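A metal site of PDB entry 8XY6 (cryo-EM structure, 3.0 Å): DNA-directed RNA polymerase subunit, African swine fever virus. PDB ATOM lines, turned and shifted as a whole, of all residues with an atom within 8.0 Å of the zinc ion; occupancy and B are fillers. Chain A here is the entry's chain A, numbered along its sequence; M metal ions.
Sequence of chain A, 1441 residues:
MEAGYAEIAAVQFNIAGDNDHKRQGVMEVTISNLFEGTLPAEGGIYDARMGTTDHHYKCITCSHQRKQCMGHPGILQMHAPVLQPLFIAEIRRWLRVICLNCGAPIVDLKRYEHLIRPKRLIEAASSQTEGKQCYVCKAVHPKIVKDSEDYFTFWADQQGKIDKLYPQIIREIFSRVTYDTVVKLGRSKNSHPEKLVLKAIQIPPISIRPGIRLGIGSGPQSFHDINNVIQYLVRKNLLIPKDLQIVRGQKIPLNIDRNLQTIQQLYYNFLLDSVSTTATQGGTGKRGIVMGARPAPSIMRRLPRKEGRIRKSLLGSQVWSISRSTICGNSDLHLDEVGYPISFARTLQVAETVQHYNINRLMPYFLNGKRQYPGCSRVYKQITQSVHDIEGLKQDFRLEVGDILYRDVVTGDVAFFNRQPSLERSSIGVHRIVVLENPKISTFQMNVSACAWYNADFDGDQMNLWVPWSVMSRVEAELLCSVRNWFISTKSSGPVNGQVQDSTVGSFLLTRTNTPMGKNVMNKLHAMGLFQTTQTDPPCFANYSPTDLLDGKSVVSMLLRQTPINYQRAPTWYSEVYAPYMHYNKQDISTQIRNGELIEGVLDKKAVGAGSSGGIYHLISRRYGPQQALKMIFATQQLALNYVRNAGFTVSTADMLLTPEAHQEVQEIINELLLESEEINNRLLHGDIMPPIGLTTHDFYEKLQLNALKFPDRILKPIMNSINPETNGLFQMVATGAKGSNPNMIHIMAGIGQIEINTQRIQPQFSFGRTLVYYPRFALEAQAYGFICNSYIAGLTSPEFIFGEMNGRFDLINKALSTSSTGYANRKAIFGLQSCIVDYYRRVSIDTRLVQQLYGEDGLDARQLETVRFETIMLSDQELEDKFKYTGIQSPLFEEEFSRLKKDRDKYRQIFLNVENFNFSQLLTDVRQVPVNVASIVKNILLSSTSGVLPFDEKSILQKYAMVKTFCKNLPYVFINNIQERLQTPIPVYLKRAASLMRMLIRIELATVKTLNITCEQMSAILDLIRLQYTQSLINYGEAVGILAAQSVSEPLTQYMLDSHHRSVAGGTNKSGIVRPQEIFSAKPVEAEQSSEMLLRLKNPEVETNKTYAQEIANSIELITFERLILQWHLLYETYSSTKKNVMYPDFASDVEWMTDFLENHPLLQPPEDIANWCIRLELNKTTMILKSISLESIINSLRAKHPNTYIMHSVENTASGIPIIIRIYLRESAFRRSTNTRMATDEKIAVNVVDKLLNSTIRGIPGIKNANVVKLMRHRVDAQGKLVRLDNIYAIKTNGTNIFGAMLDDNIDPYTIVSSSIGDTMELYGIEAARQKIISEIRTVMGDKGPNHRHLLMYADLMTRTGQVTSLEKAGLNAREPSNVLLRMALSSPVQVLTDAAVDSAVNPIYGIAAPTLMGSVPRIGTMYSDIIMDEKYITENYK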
ATOM      1  N   ILE A  98      29.795  35.160 -18.922  1.00  0.00           N
ATOM      2  CA  ILE A  98      28.660  34.351 -18.504  1.00  0.00           C
ATOM      3  C   ILE A  98      27.598  34.371 -19.590  1.00  0.00           C
ATOM      4  O   ILE A  98      27.510  35.320 -20.393  1.00  0.00           O
ATOM      5  CB  ILE A  98      28.081  34.821 -17.150  1.00  0.00           C
ATOM      6  CG1 ILE A  98      28.088  36.345 -17.045  1.00  0.00           C
ATOM      7  CG2 ILE A  98      28.880  34.245 -16.002  1.00  0.00           C
ATOM      8  CD1 ILE A  98      26.966  37.046 -17.775  1.00  0.00           C
ATOM      9  N   CYS A  99      26.802  33.311 -19.641  1.00  0.00           N
ATOM     10  CA  CYS A  99      25.761  33.190 -20.657  1.00  0.00           C
ATOM     11  C   CYS A  99      24.682  34.239 -20.419  1.00  0.00           C
ATOM     12  O   CYS A  99      24.286  34.496 -19.282  1.00  0.00           O
ATOM     13  CB  CYS A  99      25.149  31.790 -20.639  1.00  0.00           C
ATOM     14  SG  CYS A  99      23.622  31.636 -21.590  1.00  0.00           S
ATOM     15  N   LEU A 100      24.226  34.860 -21.515  1.00  0.00           N
ATOM     16  CA  LEU A 100      23.261  35.940 -21.379  1.00  0.00           C
ATOM     17  C   LEU A 100      21.888  35.407 -20.964  1.00  0.00           C
ATOM     18  O   LEU A 100      21.138  36.080 -20.253  1.00  0.00           O
ATOM     19  CB  LEU A 100      23.152  36.702 -22.700  1.00  0.00           C
ATOM     20  CG  LEU A 100      23.129  38.224 -22.587  1.00  0.00           C
ATOM     21  CD1 LEU A 100      24.000  38.670 -21.423  1.00  0.00           C
ATOM     22  CD2 LEU A 100      23.584  38.880 -23.875  1.00  0.00           C
ATOM     23  N   ASN A 101      21.549  34.188 -21.402  1.00  0.00           N
ATOM     24  CA  ASN A 101      20.213  33.653 -21.189  1.00  0.00           C
ATOM     25  C   ASN A 101      20.068  32.858 -19.902  1.00  0.00           C
ATOM     26  O   ASN A 101      18.960  32.785 -19.359  1.00  0.00           O
ATOM     27  CB  ASN A 101      19.809  32.775 -22.380  1.00  0.00           C
ATOM     28  CG  ASN A 101      19.547  33.586 -23.635  1.00  0.00           C
ATOM     29  OD1 ASN A 101      19.987  34.724 -23.755  1.00  0.00           O
ATOM     30  ND2 ASN A 101      18.826  32.988 -24.574  1.00  0.00           N
ATOM     31  N   CYS A 102      21.148  32.243 -19.413  1.00  0.00           N
ATOM     32  CA  CYS A 102      21.076  31.426 -18.214  1.00  0.00           C
ATOM     33  C   CYS A 102      22.013  31.876 -17.100  1.00  0.00           C
ATOM     34  O   CYS A 102      21.749  31.561 -15.940  1.00  0.00           O
ATOM     35  CB  CYS A 102      21.376  29.955 -18.539  1.00  0.00           C
ATOM     36  SG  CYS A 102      23.122  29.523 -18.463  1.00  0.00           S
ATOM     37  N   GLY A 103      23.099  32.587 -17.422  1.00  0.00           N
ATOM     38  CA  GLY A 103      24.001  33.102 -16.416  1.00  0.00           C
ATOM     39  C   GLY A 103      25.187  32.227 -16.100  1.00  0.00           C
ATOM     40  O   GLY A 103      26.156  32.725 -15.513  1.00  0.00           O
ATOM     41  N   ALA A 104      25.161  30.950 -16.458  1.00  0.00           N
ATOM     42  CA  ALA A 104      26.300  30.095 -16.200  1.00  0.00           C
ATOM     43  C   ALA A 104      27.470  30.520 -17.090  1.00  0.00           C
ATOM     44  O   ALA A 104      27.269  31.030 -18.194  1.00  0.00           O
ATOM     45  CB  ALA A 104      25.959  28.638 -16.458  1.00  0.00           C
ATOM     46  N   PRO A 105      28.709  30.341 -16.623  1.00  0.00           N
ATOM     47  CA  PRO A 105      29.863  30.794 -17.410  1.00  0.00           C
ATOM     48  C   PRO A 105      29.950  30.080 -18.750  1.00  0.00           C
ATOM     49  O   PRO A 105      29.655  28.885 -18.852  1.00  0.00           O
ATOM     50  CB  PRO A 105      31.061  30.471 -16.513  1.00  0.00           C
ATOM     51  CG  PRO A 105      30.574  29.367 -15.638  1.00  0.00           C
ATOM     52  CD  PRO A 105      29.119  29.645 -15.396  1.00  0.00           C
ATOM     53  N   ILE A 106      30.358  30.825 -19.775  1.00  0.00           N
ATOM     54  CA  ILE A 106      30.570  30.219 -21.082  1.00  0.00           C
ATOM     55  C   ILE A 106      32.023  29.844 -21.327  1.00  0.00           C
ATOM     56  O   ILE A 106      32.319  29.093 -22.268  1.00  0.00           O
ATOM     57  CB  ILE A 106      30.090  31.157 -22.204  1.00  0.00           C
ATOM     58  CG1 ILE A 106      30.932  32.430 -22.229  1.00  0.00           C
ATOM     59  CG2 ILE A 106      28.625  31.489 -22.029  1.00  0.00           C
ATOM     60  CD1 ILE A 106      30.455  33.436 -23.243  1.00  0.00           C
ATOM     61  N   GLN A 133      28.897  28.450 -27.649  1.00  0.00           N
ATOM     62  CA  GLN A 133      27.720  27.710 -27.209  1.00  0.00           C
ATOM     63  C   GLN A 133      27.792  27.464 -25.713  1.00  0.00           C
ATOM     64  O   GLN A 133      28.832  27.089 -25.169  1.00  0.00           O
ATOM     65  CB  GLN A 133      27.622  26.367 -27.948  1.00  0.00           C
ATOM     66  CG  GLN A 133      26.507  25.445 -27.447  1.00  0.00           C
ATOM     67  CD  GLN A 133      25.133  26.084 -27.516  1.00  0.00           C
ATOM     68  OE1 GLN A 133      24.672  26.688 -26.554  1.00  0.00           O
ATOM     69  NE2 GLN A 133      24.473  25.959 -28.668  1.00  0.00           N
ATOM     70  N   CYS A 134      26.662  27.689 -25.030  1.00  0.00           N
ATOM     71  CA  CYS A 134      26.553  27.475 -23.596  1.00  0.00           C
ATOM     72  C   CYS A 134      26.008  26.071 -23.369  1.00  0.00           C
ATOM     73  O   CYS A 134      24.867  25.771 -23.715  1.00  0.00           O
ATOM     74  CB  CYS A 134      25.648  28.524 -22.961  1.00  0.00           C
ATOM     75  SG  CYS A 134      25.107  28.109 -21.295  1.00  0.00           S
ATOM     76  N   TYR A 135      26.848  25.207 -22.788  1.00  0.00           N
ATOM     77  CA  TYR A 135      26.498  23.792 -22.680  1.00  0.00           C
ATOM     78  C   TYR A 135      25.293  23.570 -21.778  1.00  0.00           C
ATOM     79  O   TYR A 135      24.404  22.765 -22.098  1.00  0.00           O
ATOM     80  CB  TYR A 135      27.707  23.002 -22.170  1.00  0.00           C
ATOM     81  CG  TYR A 135      27.921  21.695 -22.900  1.00  0.00           C
ATOM     82  CD1 TYR A 135      26.984  21.227 -23.815  1.00  0.00           C
ATOM     83  CD2 TYR A 135      29.043  20.921 -22.663  1.00  0.00           C
ATOM     84  CE1 TYR A 135      27.174  20.034 -24.477  1.00  0.00           C
ATOM     85  CE2 TYR A 135      29.236  19.730 -23.315  1.00  0.00           C
ATOM     86  CZ  TYR A 135      28.295  19.286 -24.226  1.00  0.00           C
ATOM     87  OH  TYR A 135      28.485  18.093 -24.888  1.00  0.00           O
ATOM     88  N   VAL A 136      25.248  24.269 -20.648  1.00  0.00           N
ATOM     89  CA  VAL A 136      24.272  23.937 -19.608  1.00  0.00           C
ATOM     90  C   VAL A 136      22.852  24.255 -20.041  1.00  0.00           C
ATOM     91  O   VAL A 136      21.909  23.567 -19.643  1.00  0.00           O
ATOM     92  CB  VAL A 136      24.646  24.639 -18.292  1.00  0.00           C
ATOM     93  CG1 VAL A 136      26.102  24.354 -17.931  1.00  0.00           C
ATOM     94  CG2 VAL A 136      24.411  26.132 -18.397  1.00  0.00           C
ATOM     95  N   CYS A 137      22.661  25.305 -20.849  1.00  0.00           N
ATOM     96  CA  CYS A 137      21.324  25.741 -21.210  1.00  0.00           C
ATOM     97  C   CYS A 137      21.084  25.765 -22.715  1.00  0.00           C
ATOM     98  O   CYS A 137      19.982  26.140 -23.137  1.00  0.00           O
ATOM     99  CB  CYS A 137      21.041  27.136 -20.629  1.00  0.00           C
ATOM    100  SG  CYS A 137      21.398  28.527 -21.730  1.00  0.00           S
ATOM    101  N   LYS A 138      22.048  25.330 -23.530  1.00  0.00           N
ATOM    102  CA  LYS A 138      21.909  25.257 -24.987  1.00  0.00           C
ATOM    103  C   LYS A 138      21.407  26.582 -25.556  1.00  0.00           C
ATOM    104  O   LYS A 138      20.321  26.689 -26.125  1.00  0.00           O
ATOM    105  CB  LYS A 138      20.996  24.102 -25.399  1.00  0.00           C
ATOM    106  CG  LYS A 138      20.846  22.984 -24.368  1.00  0.00           C
ATOM    107  CD  LYS A 138      22.102  22.135 -24.281  1.00  0.00           C
ATOM    108  CE  LYS A 138      21.917  20.966 -23.322  1.00  0.00           C
ATOM    109  NZ  LYS A 138      23.118  20.090 -23.278  1.00  0.00           N
ATOM    110  N   ALA A 139      22.229  27.616 -25.385  1.00  0.00           N
ATOM    111  CA  ALA A 139      21.977  28.919 -25.986  1.00  0.00           C
ATOM    112  C   ALA A 139      23.287  29.482 -26.502  1.00  0.00           C
ATOM    113  O   ALA A 139      24.295  29.470 -25.791  1.00  0.00           O
ATOM    114  CB  ALA A 139      21.347  29.880 -24.974  1.00  0.00           C
ATOM    115  N   VAL A 140      23.274  29.967 -27.741  1.00  0.00           N
ATOM    116  CA  VAL A 140      24.474  30.557 -28.324  1.00  0.00           C
ATOM    117  C   VAL A 140      24.763  31.891 -27.672  1.00  0.00           C
ATOM    118  O   VAL A 140      23.855  32.702 -27.447  1.00  0.00           O
ATOM    119  CB  VAL A 140      24.317  30.680 -29.847  1.00  0.00           C
ATOM    120  CG1 VAL A 140      22.999  31.364 -30.191  1.00  0.00           C
ATOM    121  CG2 VAL A 140      25.490  31.438 -30.453  1.00  0.00           C
ATOM    122  N   HIS A 141      26.032  32.122 -27.337  1.00  0.00           N
ATOM    123  CA  HIS A 141      26.337  33.419 -26.721  1.00  0.00           C
ATOM    124  C   HIS A 141      26.581  34.477 -27.789  1.00  0.00           C
ATOM    125  O   HIS A 141      27.284  34.219 -28.776  1.00  0.00           O
ATOM    126  CB  HIS A 141      27.556  33.319 -25.821  1.00  0.00           C
ATOM    127  CG  HIS A 141      27.789  34.550 -24.996  1.00  0.00           C
ATOM    128  ND1 HIS A 141      28.560  35.614 -25.444  1.00  0.00           N
ATOM    129  CD2 HIS A 141      27.339  34.911 -23.770  1.00  0.00           C
ATOM    130  CE1 HIS A 141      28.576  36.552 -24.520  1.00  0.00           C
ATOM    131  NE2 HIS A 141      27.841  36.152 -23.497  1.00  0.00           N
HETATM  132 ZN    ZN M   1      23.306  29.473 -20.781  1.00  0.00          ZN
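The zinc ion is bound by the side-chain sulfur (SG) of Cys 134, the side-chain sulfur (SG) of Cys 102, the side-chain sulfur (SG) of Cys 137 and the side-chain sulfur (SG) of Cys 99.
N of Cys 134 sits at hydrogen-bond distance from O of Ala 139, at 3.1 Å.
The side-chain sulfur (SG) of Cys 102 sits close to the backbone NH (N) of Ala 104.
SG of Cys 99 lies close to N of Asn 101 (3.3 Å).
The backbone carbonyl oxygen of Ala 104 sits at hydrogen-bond distance from the backbone NH of Cys 99, at 2.7 Å.
The nearest printed residue that does not touch the zinc ion is Val 136 (4.3 Å).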
